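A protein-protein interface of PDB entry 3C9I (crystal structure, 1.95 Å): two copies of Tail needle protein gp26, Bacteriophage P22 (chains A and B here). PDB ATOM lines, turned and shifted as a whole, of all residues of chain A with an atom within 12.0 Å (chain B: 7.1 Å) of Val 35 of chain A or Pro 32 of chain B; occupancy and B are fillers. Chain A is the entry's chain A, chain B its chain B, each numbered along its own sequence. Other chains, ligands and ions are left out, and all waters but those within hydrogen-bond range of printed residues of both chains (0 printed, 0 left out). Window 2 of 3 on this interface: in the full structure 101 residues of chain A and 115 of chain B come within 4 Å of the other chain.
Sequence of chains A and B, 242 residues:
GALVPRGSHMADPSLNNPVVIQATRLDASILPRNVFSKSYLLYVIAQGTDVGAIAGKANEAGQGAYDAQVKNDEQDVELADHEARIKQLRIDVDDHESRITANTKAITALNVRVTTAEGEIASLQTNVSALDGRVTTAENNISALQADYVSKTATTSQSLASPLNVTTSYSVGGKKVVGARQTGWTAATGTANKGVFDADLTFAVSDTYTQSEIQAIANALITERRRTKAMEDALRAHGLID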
ATOM      1  N   ALA A  28      22.508   0.513   5.931  1.00  0.00           N
ATOM      2  CA  ALA A  28      23.140   1.440   6.892  1.00  0.00           C
ATOM      3  C   ALA A  28      22.283   2.658   7.261  1.00  0.00           C
ATOM      4  O   ALA A  28      22.757   3.593   7.914  1.00  0.00           O
ATOM      5  CB  ALA A  28      24.504   1.906   6.362  1.00  0.00           C
ATOM      6  N   SER A  29      21.023   2.639   6.840  1.00  0.00           N
ATOM      7  CA  SER A  29      20.093   3.723   7.130  1.00  0.00           C
ATOM      8  C   SER A  29      18.988   3.143   7.996  1.00  0.00           C
ATOM      9  O   SER A  29      18.099   3.859   8.455  1.00  0.00           O
ATOM     10  CB  SER A  29      19.496   4.302   5.839  1.00  0.00           C
ATOM     11  OG  SER A  29      18.646   3.373   5.179  1.00  0.00           O
ATOM     12  N   ILE A  30      19.055   1.831   8.203  1.00  0.00           N
ATOM     13  CA  ILE A  30      18.081   1.134   9.029  1.00  0.00           C
ATOM     14  C   ILE A  30      18.733   0.841  10.379  1.00  0.00           C
ATOM     15  O   ILE A  30      18.080   0.381  11.316  1.00  0.00           O
ATOM     16  CB  ILE A  30      17.637  -0.196   8.387  1.00  0.00           C
ATOM     17  CG1 ILE A  30      18.799  -1.189   8.382  1.00  0.00           C
ATOM     18  CG2 ILE A  30      17.163   0.047   6.961  1.00  0.00           C
ATOM     19  CD1 ILE A  30      18.418  -2.564   7.891  1.00  0.00           C
ATOM     20  N   LEU A  31      20.030   1.124  10.468  1.00  0.00           N
ATOM     21  CA  LEU A  31      20.781   0.890  11.698  1.00  0.00           C
ATOM     22  C   LEU A  31      20.567   2.015  12.713  1.00  0.00           C
ATOM     23  O   LEU A  31      20.339   3.162  12.343  1.00  0.00           O
ATOM     24  CB  LEU A  31      22.277   0.774  11.392  1.00  0.00           C
ATOM     25  CG  LEU A  31      22.753  -0.378  10.509  1.00  0.00           C
ATOM     26  CD1 LEU A  31      24.227  -0.221  10.221  1.00  0.00           C
ATOM     27  CD2 LEU A  31      22.502  -1.690  11.194  1.00  0.00           C
ATOM     28  N   PRO A  32      20.655   1.693  14.012  1.00  0.00           N
ATOM     29  CA  PRO A  32      20.470   2.685  15.072  1.00  0.00           C
ATOM     30  C   PRO A  32      21.711   3.547  15.275  1.00  0.00           C
ATOM     31  O   PRO A  32      22.790   3.033  15.563  1.00  0.00           O
ATOM     32  CB  PRO A  32      20.188   1.837  16.315  1.00  0.00           C
ATOM     33  CG  PRO A  32      19.961   0.447  15.799  1.00  0.00           C
ATOM     34  CD  PRO A  32      20.816   0.351  14.590  1.00  0.00           C
ATOM     35  N   ARG A  33      21.555   4.856  15.117  1.00  0.00           N
ATOM     36  CA  ARG A  33      22.656   5.784  15.328  1.00  0.00           C
ATOM     37  C   ARG A  33      22.620   6.228  16.793  1.00  0.00           C
ATOM     38  O   ARG A  33      21.545   6.386  17.379  1.00  0.00           O
ATOM     39  CB  ARG A  33      22.516   6.996  14.399  1.00  0.00           C
ATOM     40  CG  ARG A  33      23.456   6.999  13.189  1.00  0.00           C
ATOM     41  CD  ARG A  33      23.569   5.614  12.566  1.00  0.00           C
ATOM     42  NE  ARG A  33      23.853   5.641  11.131  1.00  0.00           N
ATOM     43  CZ  ARG A  33      24.963   6.122  10.578  1.00  0.00           C
ATOM     44  NH1 ARG A  33      25.930   6.634  11.329  1.00  0.00           N
ATOM     45  NH2 ARG A  33      25.108   6.081   9.260  1.00  0.00           N
ATOM     46  N   ASN A  34      23.798   6.408  17.383  1.00  0.00           N
ATOM     47  CA  ASN A  34      23.922   6.832  18.776  1.00  0.00           C
ATOM     48  C   ASN A  34      23.517   5.755  19.781  1.00  0.00           C
ATOM     49  O   ASN A  34      22.897   6.033  20.808  1.00  0.00           O
ATOM     50  CB  ASN A  34      23.114   8.113  19.006  1.00  0.00           C
ATOM     51  CG  ASN A  34      23.762   9.327  18.363  1.00  0.00           C
ATOM     52  OD1 ASN A  34      24.580   9.199  17.453  1.00  0.00           O
ATOM     53  ND2 ASN A  34      23.390  10.512  18.826  1.00  0.00           N
ATOM     54  N   VAL A  35      23.884   4.520  19.464  1.00  0.00           N
ATOM     55  CA  VAL A  35      23.612   3.363  20.307  1.00  0.00           C
ATOM     56  C   VAL A  35      24.692   2.340  19.976  1.00  0.00           C
ATOM     57  O   VAL A  35      25.112   1.567  20.835  1.00  0.00           O
ATOM     58  CB  VAL A  35      22.196   2.787  20.045  1.00  0.00           C
ATOM     59  CG1 VAL A  35      21.696   3.246  18.698  1.00  0.00           C
ATOM     60  CG2 VAL A  35      22.217   1.264  20.115  1.00  0.00           C
ATOM     61  N   PHE A  36      25.137   2.348  18.721  1.00  0.00           N
ATOM     62  CA  PHE A  36      26.205   1.460  18.263  1.00  0.00           C
ATOM     63  C   PHE A  36      27.432   2.341  18.120  1.00  0.00           C
ATOM     64  O   PHE A  36      27.356   3.417  17.533  1.00  0.00           O
ATOM     65  CB  PHE A  36      25.901   0.852  16.882  1.00  0.00           C
ATOM     66  CG  PHE A  36      24.884  -0.261  16.893  1.00  0.00           C
ATOM     67  CD1 PHE A  36      24.557  -0.914  15.714  1.00  0.00           C
ATOM     68  CD2 PHE A  36      24.251  -0.647  18.066  1.00  0.00           C
ATOM     69  CE1 PHE A  36      23.615  -1.940  15.698  1.00  0.00           C
ATOM     70  CE2 PHE A  36      23.310  -1.669  18.062  1.00  0.00           C
ATOM     71  CZ  PHE A  36      22.989  -2.316  16.876  1.00  0.00           C
ATOM     72  N   SER A  37      28.559   1.894  18.659  1.00  0.00           N
ATOM     73  CA  SER A  37      29.797   2.652  18.543  1.00  0.00           C
ATOM     74  C   SER A  37      30.116   2.749  17.060  1.00  0.00           C
ATOM     75  O   SER A  37      29.472   2.093  16.239  1.00  0.00           O
ATOM     76  CB  SER A  37      30.932   1.920  19.258  1.00  0.00           C
ATOM     77  OG  SER A  37      31.108   0.613  18.729  1.00  0.00           O
ATOM     78  N   LYS A  38      31.104   3.561  16.704  1.00  0.00           N
ATOM     79  CA  LYS A  38      31.475   3.691  15.303  1.00  0.00           C
ATOM     80  C   LYS A  38      32.014   2.364  14.772  1.00  0.00           C
ATOM     81  O   LYS A  38      31.635   1.916  13.688  1.00  0.00           O
ATOM     82  CB  LYS A  38      32.526   4.789  15.121  1.00  0.00           C
ATOM     83  CG  LYS A  38      33.139   4.810  13.731  1.00  0.00           C
ATOM     84  CD  LYS A  38      33.902   6.093  13.460  1.00  0.00           C
ATOM     85  CE  LYS A  38      34.692   5.992  12.158  1.00  0.00           C
ATOM     86  NZ  LYS A  38      33.846   5.570  11.006  1.00  0.00           N
ATOM     87  N   SER A  39      32.893   1.739  15.548  1.00  0.00           N
ATOM     88  CA  SER A  39      33.486   0.469  15.163  1.00  0.00           C
ATOM     89  C   SER A  39      32.448  -0.618  14.915  1.00  0.00           C
ATOM     90  O   SER A  39      32.398  -1.204  13.831  1.00  0.00           O
ATOM     91  CB  SER A  39      34.470   0.013  16.230  1.00  0.00           C
ATOM     92  OG  SER A  39      35.671   0.756  16.137  1.00  0.00           O
ATOM     93  N   TYR A  40      31.619  -0.894  15.914  1.00  0.00           N
ATOM     94  CA  TYR A  40      30.592  -1.912  15.760  1.00  0.00           C
ATOM     95  C   TYR A  40      29.745  -1.613  14.525  1.00  0.00           C
ATOM     96  O   TYR A  40      29.175  -2.519  13.911  1.00  0.00           O
ATOM     97  CB  TYR A  40      29.703  -1.962  17.000  1.00  0.00           C
ATOM     98  CG  TYR A  40      28.705  -3.088  16.977  1.00  0.00           C
ATOM     99  CD1 TYR A  40      29.114  -4.401  16.740  1.00  0.00           C
ATOM    100  CD2 TYR A  40      27.349  -2.849  17.184  1.00  0.00           C
ATOM    101  CE1 TYR A  40      28.200  -5.442  16.710  1.00  0.00           C
ATOM    102  CE2 TYR A  40      26.424  -3.891  17.153  1.00  0.00           C
ATOM    103  CZ  TYR A  40      26.862  -5.188  16.914  1.00  0.00           C
ATOM    104  OH  TYR A  40      25.964  -6.225  16.859  1.00  0.00           O
ATOM    105  N   LEU A  41      29.673  -0.335  14.163  1.00  0.00           N
ATOM    106  CA  LEU A  41      28.902   0.085  13.000  1.00  0.00           C
ATOM    107  C   LEU A  41      29.599  -0.421  11.744  1.00  0.00           C
ATOM    108  O   LEU A  41      28.968  -1.017  10.875  1.00  0.00           O
ATOM    109  CB  LEU A  41      28.794   1.611  12.956  1.00  0.00           C
ATOM    110  CG  LEU A  41      27.409   2.200  12.667  1.00  0.00           C
ATOM    111  CD1 LEU A  41      27.510   3.712  12.661  1.00  0.00           C
ATOM    112  CD2 LEU A  41      26.877   1.692  11.335  1.00  0.00           C
ATOM    113  N   LEU A  42      30.903  -0.177  11.646  1.00  0.00           N
ATOM    114  CA  LEU A  42      31.670  -0.641  10.498  1.00  0.00           C
ATOM    115  C   LEU A  42      31.650  -2.170  10.455  1.00  0.00           C
ATOM    116  O   LEU A  42      31.564  -2.776   9.384  1.00  0.00           O
ATOM    117  CB  LEU A  42      33.117  -0.148  10.587  1.00  0.00           C
ATOM    118  CG  LEU A  42      33.331   1.365  10.494  1.00  0.00           C
ATOM    119  CD1 LEU A  42      34.790   1.701  10.753  1.00  0.00           C
ATOM    120  CD2 LEU A  42      32.905   1.855   9.118  1.00  0.00           C
ATOM    121  N   TYR A  43      31.727  -2.786  11.631  1.00  0.00           N
ATOM    122  CA  TYR A  43      31.717  -4.240  11.752  1.00  0.00           C
ATOM    123  C   TYR A  43      30.426  -4.833  11.197  1.00  0.00           C
ATOM    124  O   TYR A  43      30.448  -5.767  10.395  1.00  0.00           O
ATOM    125  CB  TYR A  43      31.849  -4.635  13.222  1.00  0.00           C
ATOM    126  CG  TYR A  43      31.771  -6.125  13.482  1.00  0.00           C
ATOM    127  CD1 TYR A  43      32.904  -6.933  13.402  1.00  0.00           C
ATOM    128  CD2 TYR A  43      30.557  -6.724  13.819  1.00  0.00           C
ATOM    129  CE1 TYR A  43      32.829  -8.304  13.656  1.00  0.00           C
ATOM    130  CE2 TYR A  43      30.473  -8.088  14.073  1.00  0.00           C
ATOM    131  CZ  TYR A  43      31.611  -8.870  13.991  1.00  0.00           C
ATOM    132  OH  TYR A  43      31.525 -10.213  14.274  1.00  0.00           O
ATOM    133  N   VAL A  44      29.302  -4.292  11.644  1.00  0.00           N
ATOM    134  CA  VAL A  44      27.994  -4.769  11.215  1.00  0.00           C
ATOM    135  C   VAL A  44      27.770  -4.699   9.703  1.00  0.00           C
ATOM    136  O   VAL A  44      27.026  -5.505   9.143  1.00  0.00           O
ATOM    137  CB  VAL A  44      26.883  -3.992  11.941  1.00  0.00           C
ATOM    138  CG1 VAL A  44      25.550  -4.197  11.247  1.00  0.00           C
ATOM    139  CG2 VAL A  44      26.796  -4.468  13.382  1.00  0.00           C
ATOM    140  N   GLN A  47      30.361  -7.439   8.248  1.00  0.00           N
ATOM    141  CA  GLN A  47      29.863  -8.789   8.473  1.00  0.00           C
ATOM    142  C   GLN A  47      28.706  -9.061   7.512  1.00  0.00           C
ATOM    143  O   GLN A  47      28.411 -10.208   7.174  1.00  0.00           O
ATOM    144  CB  GLN A  47      29.386  -8.966   9.911  1.00  0.00           C
ATOM    145  CG  GLN A  47      28.900 -10.371  10.189  1.00  0.00           C
ATOM    146  CD  GLN A  47      29.060 -10.764  11.637  1.00  0.00           C
ATOM    147  OE1 GLN A  47      28.256 -10.389  12.489  1.00  0.00           O
ATOM    148  NE2 GLN A  47      30.117 -11.519  11.928  1.00  0.00           N
ATOM    149  N   ALA B  28      34.626  -7.246  22.635  1.00  0.00           N
ATOM    150  CA  ALA B  28      33.491  -6.859  23.459  1.00  0.00           C
ATOM    151  C   ALA B  28      33.420  -5.352  23.704  1.00  0.00           C
ATOM    152  O   ALA B  28      32.335  -4.777  23.725  1.00  0.00           O
ATOM    153  CB  ALA B  28      33.548  -7.603  24.788  1.00  0.00           C
ATOM    154  N   SER B  29      34.579  -4.719  23.868  1.00  0.00           N
ATOM    155  CA  SER B  29      34.656  -3.284  24.141  1.00  0.00           C
ATOM    156  C   SER B  29      34.060  -2.332  23.101  1.00  0.00           C
ATOM    157  O   SER B  29      34.072  -1.119  23.314  1.00  0.00           O
ATOM    158  CB  SER B  29      36.108  -2.878  24.395  1.00  0.00           C
ATOM    159  OG  SER B  29      36.659  -3.601  25.478  1.00  0.00           O
ATOM    160  N   ILE B  30      33.553  -2.850  21.982  1.00  0.00           N
ATOM    161  CA  ILE B  30      32.959  -1.979  20.972  1.00  0.00           C
ATOM    162  C   ILE B  30      31.441  -2.137  20.979  1.00  0.00           C
ATOM    163  O   ILE B  30      30.717  -1.367  20.326  1.00  0.00           O
ATOM    164  CB  ILE B  30      33.482  -2.284  19.543  1.00  0.00           C
ATOM    165  CG1 ILE B  30      32.944  -3.628  19.058  1.00  0.00           C
ATOM    166  CG2 ILE B  30      35.003  -2.281  19.534  1.00  0.00           C
ATOM    167  CD1 ILE B  30      33.064  -3.816  17.557  1.00  0.00           C
ATOM    168  N   LEU B  31      30.961  -3.134  21.717  1.00  0.00           N
ATOM    169  CA  LEU B  31      29.538  -3.406  21.821  1.00  0.00           C
ATOM    170  C   LEU B  31      28.843  -2.487  22.829  1.00  0.00           C
ATOM    171  O   LEU B  31      29.471  -1.945  23.734  1.00  0.00           O
ATOM    172  CB  LEU B  31      29.319  -4.871  22.250  1.00  0.00           C
ATOM    173  CG  LEU B  31      29.773  -5.937  21.261  1.00  0.00           C
ATOM    174  CD1 LEU B  31      29.687  -7.296  21.936  1.00  0.00           C
ATOM    175  CD2 LEU B  31      28.897  -5.859  20.039  1.00  0.00           C
ATOM    176  N   PRO B  32      27.514  -2.314  22.681  1.00  0.00           N
ATOM    177  CA  PRO B  32      26.658  -1.480  23.542  1.00  0.00           C
ATOM    178  C   PRO B  32      26.394  -2.184  24.875  1.00  0.00           C
ATOM    179  O   PRO B  32      25.360  -2.818  25.043  1.00  0.00           O
ATOM    180  CB  PRO B  32      25.366  -1.331  22.732  1.00  0.00           C
ATOM    181  CG  PRO B  32      25.795  -1.599  21.310  1.00  0.00           C
ATOM    182  CD  PRO B  32      26.785  -2.716  21.465  1.00  0.00           C
ATOM    183  N   ARG B  33      27.283  -2.067  25.849  1.00  0.00           N
ATOM    184  CA  ARG B  33      27.014  -2.755  27.110  1.00  0.00           C
ATOM    185  C   ARG B  33      25.709  -2.384  27.851  1.00  0.00           C
ATOM    186  O   ARG B  33      25.070  -3.268  28.450  1.00  0.00           O
ATOM    187  CB  ARG B  33      28.211  -2.606  28.081  1.00  0.00           C
ATOM    188  CG  ARG B  33      27.893  -3.204  29.467  1.00  0.00           C
ATOM    189  CD  ARG B  33      26.986  -4.463  29.354  1.00  0.00           C
ATOM    190  NE  ARG B  33      26.256  -4.757  30.599  1.00  0.00           N
ATOM    191  CZ  ARG B  33      25.100  -5.429  30.657  1.00  0.00           C
ATOM    192  NH1 ARG B  33      24.528  -5.871  29.539  1.00  0.00           N
ATOM    193  NH2 ARG B  33      24.527  -5.687  31.838  1.00  0.00           N
ATOM    194  N   ASN B  34      25.291  -1.127  27.833  1.00  0.00           N
ATOM    195  CA  ASN B  34      24.068  -0.813  28.559  1.00  0.00           C
ATOM    196  C   ASN B  34      22.797  -1.310  27.912  1.00  0.00           C
ATOM    197  O   ASN B  34      21.824  -1.647  28.568  1.00  0.00           O
ATOM    198  CB  ASN B  34      23.914   0.717  28.722  1.00  0.00           C
ATOM    199  CG  ASN B  34      24.847   1.289  29.736  1.00  0.00           C
ATOM    200  OD1 ASN B  34      25.602   0.564  30.413  1.00  0.00           O
ATOM    201  ND2 ASN B  34      24.817   2.591  29.857  1.00  0.00           N
ATOM    202  N   VAL B  35      22.823  -1.316  26.596  1.00  0.00           N
ATOM    203  CA  VAL B  35      21.639  -1.666  25.801  1.00  0.00           C
ATOM    204  C   VAL B  35      21.322  -3.098  25.306  1.00  0.00           C
ATOM    205  O   VAL B  35      20.145  -3.424  25.087  1.00  0.00           O
ATOM    206  CB  VAL B  35      21.615  -0.672  24.621  1.00  0.00           C
ATOM    207  CG1 VAL B  35      22.795   0.261  24.767  1.00  0.00           C
ATOM    208  CG2 VAL B  35      21.663  -1.393  23.307  1.00  0.00           C
ATOM    209  N   PHE B  36      22.325  -3.962  25.161  1.00  0.00           N
ATOM    210  CA  PHE B  36      22.092  -5.344  24.713  1.00  0.00           C
ATOM    211  C   PHE B  36      22.093  -6.211  25.954  1.00  0.00           C
ATOM    212  O   PHE B  36      22.866  -5.977  26.884  1.00  0.00           O
ATOM    213  CB  PHE B  36      23.231  -5.824  23.811  1.00  0.00           C
ATOM    214  CG  PHE B  36      23.270  -5.187  22.438  1.00  0.00           C
ATOM    215  CD1 PHE B  36      22.378  -4.190  22.058  1.00  0.00           C
ATOM    216  CD2 PHE B  36      24.225  -5.607  21.520  1.00  0.00           C
ATOM    217  CE1 PHE B  36      22.442  -3.632  20.782  1.00  0.00           C
ATOM    218  CE2 PHE B  36      24.293  -5.056  20.251  1.00  0.00           C
ATOM    219  CZ  PHE B  36      23.403  -4.070  19.884  1.00  0.00           C
ATOM    220  N   SER B  37      21.229  -7.212  25.966  1.00  0.00           N
ATOM    221  CA  SER B  37      21.171  -8.137  27.087  1.00  0.00           C
ATOM    222  C   SER B  37      22.502  -8.896  27.109  1.00  0.00           C
ATOM    223  O   SER B  37      23.331  -8.734  26.205  1.00  0.00           O
ATOM    224  CB  SER B  37      20.029  -9.131  26.890  1.00  0.00           C
ATOM    225  OG  SER B  37      20.142 -10.226  27.785  1.00  0.00           O
ATOM    226  N   LEU B  41      24.555 -10.384  23.929  1.00  0.00           N
ATOM    227  CA  LEU B  41      25.964 -10.015  23.864  1.00  0.00           C
ATOM    228  C   LEU B  41      26.755 -11.279  23.517  1.00  0.00           C
ATOM    229  O   LEU B  41      27.697 -11.247  22.722  1.00  0.00           O
ATOM    230  CB  LEU B  41      26.405  -9.467  25.223  1.00  0.00           C
ATOM    231  CG  LEU B  41      27.133  -8.124  25.310  1.00  0.00           C
ATOM    232  CD1 LEU B  41      26.410  -7.062  24.500  1.00  0.00           C
ATOM    233  CD2 LEU B  41      27.213  -7.718  26.772  1.00  0.00           C
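The side-chain hydroxyl (OG) of Ser 37 of chain A sits at hydrogen-bond distance from the backbone carbonyl oxygen (O) of Ile 30 of chain B (2.6 Å).
NH1 of Arg 33 of chain B lies within hydrogen-bond range of O of Phe 36 of chain B (3.1 Å). N of Tyr 40 of chain A is in hydrogen-bond range of OG of Ser 37 of chain A (3.2 Å).
Among the printed residues, pairs that only touch across the chains: Phe 36 of chain A with Phe 36 of chain B, Val 35 of chain A with Pro 32 of chain B, Tyr 40 of chain A with Leu 31 of chain B, Tyr 40 of chain A with Ile 30 of chain B, Phe 36 of chain A with Pro 32 of chain B and Tyr 40 of chain A with Phe 36 of chain B.
Pro 32 of chain A touches none of the printed residues of chain B. Of chain B, only Pro 32 (3.3 Å) comes within 4 Å of Val 35 of chain A. Of the printed residues of chain B, Phe 36 of chain A touches Pro 32 and Phe 36. Printed residues of chain B within 4 Å of Ser 37 of chain A: Ile 30. Printed residues of chain B within 4 Å of Tyr 40 of chain A: Ile 30, Leu 31 and Phe 36. Leu 31 of chain B touches just one residue of chain A: Tyr 40. Of chain A, only Val 35 and Phe 36 come within 4 Å of Pro 32 of chain B. No residue of chain A comes within 4 Å of Arg 33 of chain B. No residue of chain A comes within 4 Å of Asn 34 of chain B. No residue of chain A comes within 4 Å of Val 35 of chain B. Phe 36 of chain B touches two residues of chain A. The nearest residue of chain B that does not touch Val 35 of chain A is Val 35 of chain B (4.2 Å). The nearest residue of chain A that does not touch Pro 32 of chain B is Tyr 40 of chain A (4.3 Å). The nearest printed residue of chain B that does not touch Tyr 40 of chain A is Pro 32 of chain B (4.3 Å).
Hydrophobic or aromatic side chains of chain B that line the printed part of chain A: Ile 30, Leu 31, Pro 32 and Phe 36. Of the 18 printed residues of chain A, 4 touch a printed residue of chain B. Hydrophobic or aromatic side chains of chain A that line the printed part of chain B: Phe 36 and Tyr 40. Among the printed residues, 7 pairs touch across the chains. Among the printed residues, no Asp or Glu carboxylate lies within 4 Å of a Lys or Arg side-chain nitrogen of the other chain.
Val 35 of chain A touches Pro 32 of chain B, but with the chains exchanged Pro 32 of chain A does not touch Val 35 of chain B (7.8 Å). Phe 36 of chain A touches Pro 32 of chain B, but with the chains exchanged Pro 32 of chain A does not touch Phe 36 of chain B (6.9 Å). Phe 36 of chain A touches its own counterpart, Phe 36 of chain B. Ser 37 of chain A touches Ile 30 of chain B, but with the chains exchanged Ile 30 of chain A does not touch Ser 37 of chain B (16.8 Å). Positions printed for both chains: 28, 29, 30, 31, 32, 33, 34, 35, 36, 37 and 41. Of the 7 pairs that touch across the chains among the printed residues, 1 has its exchanged pair printed and touching as well.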
